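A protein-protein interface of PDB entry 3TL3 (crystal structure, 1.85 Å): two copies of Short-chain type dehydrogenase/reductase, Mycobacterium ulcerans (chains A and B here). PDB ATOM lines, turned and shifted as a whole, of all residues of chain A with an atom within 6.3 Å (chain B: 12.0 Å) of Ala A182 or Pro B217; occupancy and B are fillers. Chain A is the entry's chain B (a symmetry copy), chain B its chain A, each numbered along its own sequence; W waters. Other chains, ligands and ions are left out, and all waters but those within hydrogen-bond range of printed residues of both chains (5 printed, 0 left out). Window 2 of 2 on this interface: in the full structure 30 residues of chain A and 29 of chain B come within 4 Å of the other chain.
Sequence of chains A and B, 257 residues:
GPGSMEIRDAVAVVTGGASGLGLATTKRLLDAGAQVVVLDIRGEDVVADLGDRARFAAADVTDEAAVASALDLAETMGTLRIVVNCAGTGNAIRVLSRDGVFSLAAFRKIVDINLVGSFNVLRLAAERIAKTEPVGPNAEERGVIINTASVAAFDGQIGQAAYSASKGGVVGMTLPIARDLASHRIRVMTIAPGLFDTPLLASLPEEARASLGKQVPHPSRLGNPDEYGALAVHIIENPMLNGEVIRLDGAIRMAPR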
ATOM      1  N   ILE A 177      17.065  16.557  35.548  1.00  0.00           N
ATOM      2  CA  ILE A 177      17.245  18.007  35.663  1.00  0.00           C
ATOM      3  C   ILE A 177      18.608  18.448  35.104  1.00  0.00           C
ATOM      4  O   ILE A 177      18.681  19.441  34.374  1.00  0.00           O
ATOM      5  CB  ILE A 177      17.020  18.486  37.105  1.00  0.00           C
ATOM      6  CG1 ILE A 177      15.549  18.286  37.505  1.00  0.00           C
ATOM      7  CG2 ILE A 177      17.359  19.963  37.251  1.00  0.00           C
ATOM      8  CD1 ILE A 177      15.277  18.667  38.945  1.00  0.00           C
ATOM      9  N   ALA A 178      19.672  17.709  35.402  1.00  0.00           N
ATOM     10  CA  ALA A 178      20.969  18.006  34.771  1.00  0.00           C
ATOM     11  C   ALA A 178      20.866  18.063  33.252  1.00  0.00           C
ATOM     12  O   ALA A 178      21.413  18.977  32.603  1.00  0.00           O
ATOM     13  CB  ALA A 178      22.022  16.992  35.183  1.00  0.00           C
ATOM     14  N   ARG A 179      20.163  17.099  32.677  1.00  0.00           N
ATOM     15  CA  ARG A 179      19.995  17.075  31.220  1.00  0.00           C
ATOM     16  C   ARG A 179      19.175  18.251  30.699  1.00  0.00           C
ATOM     17  O   ARG A 179      19.529  18.817  29.664  1.00  0.00           O
ATOM     18  CB  ARG A 179      19.442  15.735  30.755  1.00  0.00           C
ATOM     19  CG  ARG A 179      20.518  14.664  30.910  1.00  0.00           C
ATOM     20  CD  ARG A 179      20.084  13.304  30.422  1.00  0.00           C
ATOM     21  NE  ARG A 179      21.185  12.330  30.520  1.00  0.00           N
ATOM     22  CZ  ARG A 179      21.006  11.009  30.592  1.00  0.00           C
ATOM     23  NH1 ARG A 179      19.774  10.492  30.569  1.00  0.00           N
ATOM     24  NH2 ARG A 179      22.055  10.193  30.685  1.00  0.00           N
ATOM     25  N   ASP A 180      18.122  18.639  31.418  1.00  0.00           N
ATOM     26  CA  ASP A 180      17.317  19.802  31.027  1.00  0.00           C
ATOM     27  C   ASP A 180      18.048  21.136  31.203  1.00  0.00           C
ATOM     28  O   ASP A 180      17.784  22.083  30.471  1.00  0.00           O
ATOM     29  CB  ASP A 180      15.980  19.827  31.771  1.00  0.00           C
ATOM     30  CG  ASP A 180      15.011  18.748  31.301  1.00  0.00           C
ATOM     31  OD1 ASP A 180      15.185  18.201  30.185  1.00  0.00           O
ATOM     32  OD2 ASP A 180      14.050  18.445  32.045  1.00  0.00           O
ATOM     33  N   LEU A 181      18.982  21.209  32.145  1.00  0.00           N
ATOM     34  CA  LEU A 181      19.753  22.444  32.370  1.00  0.00           C
ATOM     35  C   LEU A 181      21.091  22.521  31.598  1.00  0.00           C
ATOM     36  O   LEU A 181      21.749  23.573  31.577  1.00  0.00           O
ATOM     37  CB  LEU A 181      19.974  22.646  33.873  1.00  0.00           C
ATOM     38  CG  LEU A 181      18.720  22.999  34.700  1.00  0.00           C
ATOM     39  CD1 LEU A 181      19.122  23.264  36.153  1.00  0.00           C
ATOM     40  CD2 LEU A 181      17.919  24.178  34.119  1.00  0.00           C
ATOM     41  N   ALA A 182      21.473  21.437  30.929  1.00  0.00           N
ATOM     42  CA  ALA A 182      22.710  21.391  30.151  1.00  0.00           C
ATOM     43  C   ALA A 182      22.857  22.562  29.150  1.00  0.00           C
ATOM     44  O   ALA A 182      23.909  23.202  29.066  1.00  0.00           O
ATOM     45  CB  ALA A 182      22.815  20.067  29.419  1.00  0.00           C
ATOM     46  N   SER A 183      21.799  22.846  28.410  1.00  0.00           N
ATOM     47  CA  SER A 183      21.841  23.921  27.424  1.00  0.00           C
ATOM     48  C   SER A 183      22.080  25.308  28.052  1.00  0.00           C
ATOM     49  O   SER A 183      22.464  26.254  27.339  1.00  0.00           O
ATOM     50  CB  SER A 183      20.558  23.923  26.606  1.00  0.00           C
ATOM     51  OG  SER A 183      19.463  24.320  27.401  1.00  0.00           O
ATOM     52  N   HIS A 184      21.840  25.418  29.362  1.00  0.00           N
ATOM     53  CA  HIS A 184      22.081  26.634  30.147  1.00  0.00           C
ATOM     54  C   HIS A 184      23.406  26.666  30.862  1.00  0.00           C
ATOM     55  O   HIS A 184      23.753  27.671  31.519  1.00  0.00           O
ATOM     56  CB  HIS A 184      20.939  26.822  31.157  1.00  0.00           C
ATOM     57  CG  HIS A 184      19.595  27.002  30.491  1.00  0.00           C
ATOM     58  ND1 HIS A 184      19.285  28.108  29.813  1.00  0.00           N
ATOM     59  CD2 HIS A 184      18.516  26.136  30.347  1.00  0.00           C
ATOM     60  CE1 HIS A 184      18.045  27.994  29.296  1.00  0.00           C
ATOM     61  NE2 HIS A 184      17.579  26.780  29.611  1.00  0.00           N
ATOM     62  N   ARG A 185      24.169  25.592  30.728  1.00  0.00           N
ATOM     63  CA  ARG A 185      25.504  25.496  31.330  1.00  0.00           C
ATOM     64  C   ARG A 185      25.411  25.554  32.861  1.00  0.00           C
ATOM     65  O   ARG A 185      26.223  26.189  33.532  1.00  0.00           O
ATOM     66  CB  ARG A 185      26.472  26.569  30.781  1.00  0.00           C
ATOM     67  CG  ARG A 185      26.664  26.514  29.275  1.00  0.00           C
ATOM     68  CD  ARG A 185      27.423  27.726  28.729  1.00  0.00           C
ATOM     69  NE  ARG A 185      27.650  27.584  27.290  1.00  0.00           N
ATOM     70  CZ  ARG A 185      28.567  26.771  26.746  1.00  0.00           C
ATOM     71  NH1 ARG A 185      29.367  26.021  27.504  1.00  0.00           N
ATOM     72  NH2 ARG A 185      28.678  26.702  25.427  1.00  0.00           N
ATOM     73  N   ILE A 186      24.413  24.853  33.400  1.00  0.00           N
ATOM     74  CA  ILE A 186      24.280  24.692  34.844  1.00  0.00           C
ATOM     75  C   ILE A 186      24.326  23.215  35.185  1.00  0.00           C
ATOM     76  O   ILE A 186      23.484  22.429  34.720  1.00  0.00           O
ATOM     77  CB  ILE A 186      22.955  25.275  35.363  1.00  0.00           C
ATOM     78  CG1 ILE A 186      22.859  26.762  35.001  1.00  0.00           C
ATOM     79  CG2 ILE A 186      22.882  25.108  36.886  1.00  0.00           C
ATOM     80  CD1 ILE A 186      21.467  27.334  35.171  1.00  0.00           C
ATOM     81  N   ASN A 242      28.641  15.941  36.581  1.00  0.00           N
ATOM     82  CA  ASN A 242      27.276  16.373  36.313  1.00  0.00           C
ATOM     83  C   ASN A 242      26.301  15.208  36.276  1.00  0.00           C
ATOM     84  O   ASN A 242      26.637  14.136  35.785  1.00  0.00           O
ATOM     85  CB  ASN A 242      27.262  17.119  34.987  1.00  0.00           C
ATOM     86  CG  ASN A 242      26.033  17.985  34.789  1.00  0.00           C
ATOM     87  OD1 ASN A 242      25.248  18.221  35.715  1.00  0.00           O
ATOM     88  ND2 ASN A 242      25.862  18.475  33.550  1.00  0.00           N
ATOM     89  N   PRO B 193      34.643   7.051  34.405  1.00  0.00           N
ATOM     90  CA  PRO B 193      34.721   8.204  33.516  1.00  0.00           C
ATOM     91  C   PRO B 193      33.937   8.038  32.227  1.00  0.00           C
ATOM     92  O   PRO B 193      33.790   6.920  31.719  1.00  0.00           O
ATOM     93  CB  PRO B 193      36.213   8.323  33.202  1.00  0.00           C
ATOM     94  CG  PRO B 193      36.763   6.950  33.416  1.00  0.00           C
ATOM     95  CD  PRO B 193      35.882   6.253  34.419  1.00  0.00           C
ATOM     96  N   GLY B 194      33.461   9.161  31.701  1.00  0.00           N
ATOM     97  CA  GLY B 194      32.853   9.193  30.386  1.00  0.00           C
ATOM     98  C   GLY B 194      33.924   9.359  29.328  1.00  0.00           C
ATOM     99  O   GLY B 194      35.028   8.843  29.466  1.00  0.00           O
ATOM    100  N   LEU B 195      33.600  10.131  28.306  1.00  0.00           N
ATOM    101  CA  LEU B 195      34.499  10.370  27.184  1.00  0.00           C
ATOM    102  C   LEU B 195      35.627  11.319  27.589  1.00  0.00           C
ATOM    103  O   LEU B 195      35.363  12.490  27.840  1.00  0.00           O
ATOM    104  CB  LEU B 195      33.699  10.980  26.019  1.00  0.00           C
ATOM    105  CG  LEU B 195      32.594  10.098  25.395  1.00  0.00           C
ATOM    106  CD1 LEU B 195      31.662  10.851  24.433  1.00  0.00           C
ATOM    107  CD2 LEU B 195      33.254   8.912  24.701  1.00  0.00           C
ATOM    108  N   PHE B 196      36.865  10.826  27.638  1.00  0.00           N
ATOM    109  CA  PHE B 196      38.017  11.686  27.942  1.00  0.00           C
ATOM    110  C   PHE B 196      39.012  11.838  26.789  1.00  0.00           C
ATOM    111  O   PHE B 196      39.153  10.951  25.928  1.00  0.00           O
ATOM    112  CB  PHE B 196      38.742  11.233  29.226  1.00  0.00           C
ATOM    113  CG  PHE B 196      38.169  11.824  30.487  1.00  0.00           C
ATOM    114  CD1 PHE B 196      38.870  12.767  31.231  1.00  0.00           C
ATOM    115  CD2 PHE B 196      36.914  11.442  30.924  1.00  0.00           C
ATOM    116  CE1 PHE B 196      38.331  13.296  32.403  1.00  0.00           C
ATOM    117  CE2 PHE B 196      36.363  11.976  32.071  1.00  0.00           C
ATOM    118  CZ  PHE B 196      37.077  12.907  32.821  1.00  0.00           C
ATOM    119  N   ALA B 210      35.868  15.974  17.791  1.00  0.00           N
ATOM    120  CA  ALA B 210      34.864  17.030  17.957  1.00  0.00           C
ATOM    121  C   ALA B 210      33.447  16.459  18.102  1.00  0.00           C
ATOM    122  O   ALA B 210      32.682  16.902  18.957  1.00  0.00           O
ATOM    123  CB  ALA B 210      34.920  17.998  16.778  1.00  0.00           C
ATOM    124  N   SER B 211      33.104  15.479  17.267  1.00  0.00           N
ATOM    125  CA  SER B 211      31.767  14.875  17.282  1.00  0.00           C
ATOM    126  C   SER B 211      31.491  14.146  18.592  1.00  0.00           C
ATOM    127  O   SER B 211      30.401  14.240  19.143  1.00  0.00           O
ATOM    128  CB  SER B 211      31.591  13.912  16.095  1.00  0.00           C
ATOM    129  N   LEU B 212      32.483  13.423  19.093  1.00  0.00           N
ATOM    130  CA  LEU B 212      32.356  12.744  20.386  1.00  0.00           C
ATOM    131  C   LEU B 212      32.034  13.736  21.502  1.00  0.00           C
ATOM    132  O   LEU B 212      31.115  13.514  22.296  1.00  0.00           O
ATOM    133  CB  LEU B 212      33.647  11.993  20.725  1.00  0.00           C
ATOM    134  CG  LEU B 212      33.877  10.676  19.981  1.00  0.00           C
ATOM    135  CD1 LEU B 212      35.307  10.172  20.188  1.00  0.00           C
ATOM    136  CD2 LEU B 212      32.849   9.648  20.445  1.00  0.00           C
ATOM    137  N   GLY B 213      32.797  14.829  21.548  1.00  0.00           N
ATOM    138  CA  GLY B 213      32.602  15.882  22.547  1.00  0.00           C
ATOM    139  C   GLY B 213      31.178  16.405  22.598  1.00  0.00           C
ATOM    140  O   GLY B 213      30.613  16.574  23.674  1.00  0.00           O
ATOM    141  N   LYS B 214      30.590  16.633  21.428  1.00  0.00           N
ATOM    142  CA  LYS B 214      29.227  17.179  21.298  1.00  0.00           C
ATOM    143  C   LYS B 214      28.106  16.314  21.890  1.00  0.00           C
ATOM    144  O   LYS B 214      27.058  16.840  22.231  1.00  0.00           O
ATOM    145  CB  LYS B 214      28.911  17.462  19.818  1.00  0.00           C
ATOM    146  N   GLN B 215      28.296  15.005  22.034  1.00  0.00           N
ATOM    147  CA  GLN B 215      27.222  14.192  22.629  1.00  0.00           C
ATOM    148  C   GLN B 215      27.230  14.197  24.167  1.00  0.00           C
ATOM    149  O   GLN B 215      26.358  13.599  24.805  1.00  0.00           O
ATOM    150  CB  GLN B 215      27.223  12.764  22.084  1.00  0.00           C
ATOM    151  CG  GLN B 215      28.371  11.869  22.505  1.00  0.00           C
ATOM    152  CD  GLN B 215      28.488  10.655  21.599  1.00  0.00           C
ATOM    153  OE1 GLN B 215      28.569  10.785  20.376  1.00  0.00           O
ATOM    154  NE2 GLN B 215      28.477   9.470  22.193  1.00  0.00           N
ATOM    155  N   VAL B 216      28.196  14.877  24.766  1.00  0.00           N
ATOM    156  CA  VAL B 216      28.192  15.061  26.221  1.00  0.00           C
ATOM    157  C   VAL B 216      27.289  16.265  26.535  1.00  0.00           C
ATOM    158  O   VAL B 216      27.431  17.316  25.920  1.00  0.00           O
ATOM    159  CB  VAL B 216      29.611  15.271  26.774  1.00  0.00           C
ATOM    160  CG1 VAL B 216      29.580  15.396  28.291  1.00  0.00           C
ATOM    161  CG2 VAL B 216      30.511  14.109  26.353  1.00  0.00           C
ATOM    162  N   PRO B 217      26.333  16.101  27.460  1.00  0.00           N
ATOM    163  CA  PRO B 217      25.387  17.206  27.701  1.00  0.00           C
ATOM    164  C   PRO B 217      26.041  18.489  28.176  1.00  0.00           C
ATOM    165  O   PRO B 217      25.796  19.538  27.600  1.00  0.00           O
ATOM    166  CB  PRO B 217      24.452  16.636  28.771  1.00  0.00           C
ATOM    167  CG  PRO B 217      24.418  15.173  28.433  1.00  0.00           C
ATOM    168  CD  PRO B 217      25.831  14.830  28.012  1.00  0.00           C
ATOM    169  N   HIS B 218      26.869  18.407  29.210  1.00  0.00           N
ATOM    170  CA  HIS B 218      27.496  19.599  29.758  1.00  0.00           C
ATOM    171  C   HIS B 218      28.478  19.196  30.820  1.00  0.00           C
ATOM    172  O   HIS B 218      28.105  18.523  31.789  1.00  0.00           O
ATOM    173  CB  HIS B 218      26.465  20.591  30.332  1.00  0.00           C
ATOM    174  CG  HIS B 218      27.094  21.757  31.053  1.00  0.00           C
ATOM    175  ND1 HIS B 218      27.944  22.620  30.434  1.00  0.00           N
ATOM    176  CD2 HIS B 218      26.987  22.195  32.391  1.00  0.00           C
ATOM    177  CE1 HIS B 218      28.364  23.555  31.336  1.00  0.00           C
ATOM    178  NE2 HIS B 218      27.769  23.298  32.524  1.00  0.00           N
ATOM    179  N   PRO B 219      29.752  19.576  30.653  1.00  0.00           N
ATOM    180  CA  PRO B 219      30.312  20.349  29.530  1.00  0.00           C
ATOM    181  C   PRO B 219      30.336  19.504  28.258  1.00  0.00           C
ATOM    182  O   PRO B 219      30.673  18.317  28.330  1.00  0.00           O
ATOM    183  CB  PRO B 219      31.746  20.671  29.984  1.00  0.00           C
ATOM    184  CG  PRO B 219      31.884  20.169  31.380  1.00  0.00           C
ATOM    185  CD  PRO B 219      30.797  19.151  31.600  1.00  0.00           C
ATOM    186  N   SER B 220      30.009  20.103  27.116  1.00  0.00           N
ATOM    187  CA  SER B 220      29.890  19.359  25.860  1.00  0.00           C
ATOM    188  C   SER B 220      31.238  19.306  25.166  1.00  0.00           C
ATOM    189  O   SER B 220      31.440  19.923  24.119  1.00  0.00           O
ATOM    190  CB  SER B 220      28.819  19.956  24.946  1.00  0.00           C
ATOM    191  OG  SER B 220      29.147  21.275  24.535  1.00  0.00           O
ATOM    192  N   ARG B 221      32.144  18.564  25.784  1.00  0.00           N
ATOM    193  CA  ARG B 221      33.495  18.432  25.313  1.00  0.00           C
ATOM    194  C   ARG B 221      34.051  17.180  25.936  1.00  0.00           C
ATOM    195  O   ARG B 221      33.483  16.651  26.883  1.00  0.00           O
ATOM    196  CB  ARG B 221      34.328  19.653  25.728  1.00  0.00           C
ATOM    197  CG  ARG B 221      34.250  19.967  27.215  1.00  0.00           C
ATOM    198  CD  ARG B 221      35.585  20.443  27.743  1.00  0.00           C
ATOM    199  NE  ARG B 221      35.525  20.924  29.120  1.00  0.00           N
ATOM    200  CZ  ARG B 221      35.983  20.278  30.182  1.00  0.00           C
ATOM    201  NH1 ARG B 221      36.539  19.068  30.059  1.00  0.00           N
ATOM    202  NH2 ARG B 221      35.886  20.846  31.384  1.00  0.00           N
ATOM    203  N   LEU B 222      35.162  16.694  25.402  1.00  0.00           N
ATOM    204  CA  LEU B 222      35.882  15.608  26.033  1.00  0.00           C
ATOM    205  C   LEU B 222      36.381  16.066  27.415  1.00  0.00           C
ATOM    206  O   LEU B 222      36.761  17.222  27.594  1.00  0.00           O
ATOM    207  CB  LEU B 222      37.084  15.200  25.182  1.00  0.00           C
ATOM    208  CG  LEU B 222      36.800  14.678  23.781  1.00  0.00           C
ATOM    209  CD1 LEU B 222      38.104  14.457  23.026  1.00  0.00           C
ATOM    210  CD2 LEU B 222      35.981  13.399  23.872  1.00  0.00           C
ATOM    211  N   GLY B 223      36.374  15.149  28.377  1.00  0.00           N
ATOM    212  CA  GLY B 223      36.977  15.408  29.677  1.00  0.00           C
ATOM    213  C   GLY B 223      38.476  15.585  29.542  1.00  0.00           C
ATOM    214  O   GLY B 223      39.094  14.971  28.652  1.00  0.00           O
ATOM    215  N   ARG B 247      30.484   8.639  38.934  1.00  0.00           N
ATOM    216  CA  ARG B 247      30.489   8.882  37.504  1.00  0.00           C
ATOM    217  C   ARG B 247      31.057  10.280  37.239  1.00  0.00           C
ATOM    218  O   ARG B 247      30.665  11.260  37.900  1.00  0.00           O
ATOM    219  CB  ARG B 247      29.051   8.764  36.955  1.00  0.00           C
ATOM    220  N   LEU B 248      32.000  10.363  36.306  1.00  0.00           N
ATOM    221  CA  LEU B 248      32.626  11.609  35.938  1.00  0.00           C
ATOM    222  C   LEU B 248      32.467  11.736  34.439  1.00  0.00           C
ATOM    223  O   LEU B 248      33.332  11.270  33.683  1.00  0.00           O
ATOM    224  CB  LEU B 248      34.114  11.559  36.348  1.00  0.00           C
ATOM    225  CG  LEU B 248      34.959  12.805  36.089  1.00  0.00           C
ATOM    226  CD1 LEU B 248      34.466  13.940  36.991  1.00  0.00           C
ATOM    227  CD2 LEU B 248      36.440  12.490  36.348  1.00  0.00           C
ATOM    228  N   ASP B 249      31.338  12.297  34.003  1.00  0.00           N
ATOM    229  CA  ASP B 249      30.916  12.119  32.614  1.00  0.00           C
ATOM    230  C   ASP B 249      30.008  13.191  32.012  1.00  0.00           C
ATOM    231  O   ASP B 249      29.464  12.977  30.946  1.00  0.00           O
ATOM    232  CB  ASP B 249      30.233  10.758  32.486  1.00  0.00           C
ATOM    233  CG  ASP B 249      28.913  10.675  33.227  1.00  0.00           C
ATOM    234  OD1 ASP B 249      28.356  11.705  33.689  1.00  0.00           O
ATOM    235  OD2 ASP B 249      28.424   9.538  33.335  1.00  0.00           O
ATOM    236  N   GLY B 250      29.869  14.359  32.647  1.00  0.00           N
ATOM    237  CA  GLY B 250      29.086  15.437  32.029  1.00  0.00           C
ATOM    238  C   GLY B 250      27.620  15.082  31.804  1.00  0.00           C
ATOM    239  O   GLY B 250      26.957  15.681  30.943  1.00  0.00           O
ATOM    240  N   ALA B 251      27.118  14.129  32.588  1.00  0.00           N
ATOM    241  CA  ALA B 251      25.740  13.618  32.504  1.00  0.00           C
ATOM    242  C   ALA B 251      25.434  12.844  31.225  1.00  0.00           C
ATOM    243  O   ALA B 251      24.263  12.717  30.854  1.00  0.00           O
ATOM    244  CB  ALA B 251      24.709  14.732  32.722  1.00  0.00           C
ATOM    245  N   ILE B 252      26.458  12.300  30.572  1.00  0.00           N
ATOM    246  CA  ILE B 252      26.237  11.506  29.350  1.00  0.00           C
ATOM    247  C   ILE B 252      25.538  10.165  29.636  1.00  0.00           C
ATOM    248  O   ILE B 252      24.743   9.720  28.789  1.00  0.00           O
ATOM    249  CB  ILE B 252      27.541  11.219  28.572  1.00  0.00           C
ATOM    250  CG1 ILE B 252      27.208  10.849  27.118  1.00  0.00           C
ATOM    251  CG2 ILE B 252      28.328  10.104  29.241  1.00  0.00           C
ATOM    252  CD1 ILE B 252      28.398  10.885  26.179  1.00  0.00           C
HETATM  253  O   HOH W   1      31.215  23.183  26.870  1.00  0.00           O
HETATM  254  O   HOH W   2      28.440  24.521  35.066  1.00  0.00           O
HETATM  255  O   HOH W   3      28.446  22.671  27.734  1.00  0.00           O
HETATM  256  O   HOH W   4      26.307  11.288  35.404  1.00  0.00           O
HETATM  257  O   HOH W   5      29.434  13.053  36.219  1.00  0.00           O
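Water W4 lies within hydrogen-bond range of OD1 of Asp B249 and O of Asn A242.
Water W3 lies within hydrogen-bond range of a ring nitrogen (ND1) of His B218, the backbone NH of Ser B220 and the guanidinium group of Arg A185.
Water W5 lies within hydrogen-bond range of O of Arg B247 (2.7 Å), N of Asp B249 (3.0 Å) and N of Asn A242 (3.0 Å).
Water W2 lies within hydrogen-bond range of a ring nitrogen (NE2) of His B218 (2.9 Å) and the backbone carbonyl oxygen (O) of Arg A185 (3.2 Å).
Water W1 lies within hydrogen-bond range of the backbone NH (N) of Ser B220 (3.3 Å) and the guanidinium group (NH1) of Arg A185 (3.4 Å).
O of Pro B217 touches CB of Ala A182, 3.5 Å away.
His B218 touches Ala A182.
His B218 touches Ile A186.
OD1 of Asp B249 touches O of Asn A242 (3.6 Å).
Asn A242 touches Gly B250 (CB to C, 3.8 Å).
The backbone NH (N) of His B218 sits at hydrogen-bond distance from the backbone carbonyl oxygen (O) of Gly B250 (3.2 Å).
The side-chain carboxylate of Asp B249 lies within hydrogen-bond range of the backbone NH of Ala B251, 2.9 Å away.
The backbone NH (N) of Ile A186 is in hydrogen-bond range of the backbone carbonyl oxygen (O) of Leu A181, 3.5 Å away.
Hydrophobic or aromatic side chains of chain A that line the printed part of chain B: Ala A182.
Along chain A the printed residues that touch a printed residue of chain B span positions 179 to 242.
Along chain B the printed residues that touch a printed residue of chain A span positions 217 to 252.
Among the printed residues, 10 pairs touch across the chains.
Of chain B, only Pro B217 (3.5 Å) and His B218 (3.8 Å) come within 4 Å of Ala A182.
Pro B217 touches just one residue of chain A: Ala A182.
No residue of chain B comes within 4 Å of Ala A178.
Of the printed residues of chain B, Arg A179 touches Ala B251 (3.1 Å) and Ile B252 (3.3 Å).
No residue of chain B comes within 4 Å of His A184.
Of chain B, only His B218 (3.3 Å) comes within 4 Å of Arg A185.
Of the printed residues of chain A, Asp B249 touches Asn A242 (3.6 Å).
Printed residues of chain A within 4 Å of Gly B250: Asn A242.
Printed residues of chain A within 4 Å of Ala B251: Arg A179 and Asn A242.
Gly B213 touches none of the printed residues of chain A.
Ser B220 touches none of the printed residues of chain A.
The nearest printed residue of chain B that does not touch Ala A182 is Gly B250 (6.2 Å).
The nearest residue of chain A that does not touch Pro B217 is Arg A179 (4.6 Å).
The nearest printed residue of chain B that does not touch Asn A242 is Pro B219 (5.0 Å).
NE2 of His B218 sits close to O of Arg A185, at 3.4 Å.
The side-chain amide nitrogen (ND2) of Asn A242 sits at hydrogen-bond distance from the backbone carbonyl oxygen (O) of His B218 (2.9 Å).
NE of Arg A179 lies within hydrogen-bond range of O of Ala B251, 3.1 Å away.
The backbone NH (N) of Ala B251 is in hydrogen-bond range of the backbone carbonyl oxygen (O) of Asn A242, at 3.2 Å.
The backbone carbonyl oxygen of Ile B252 lies within hydrogen-bond range of the guanidinium group of Arg A179 (3.3 Å).
No position is printed for both chains.
Of the 10 pairs that touch across the chains among the printed residues, none has its exchanged pair printed and touching as well.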
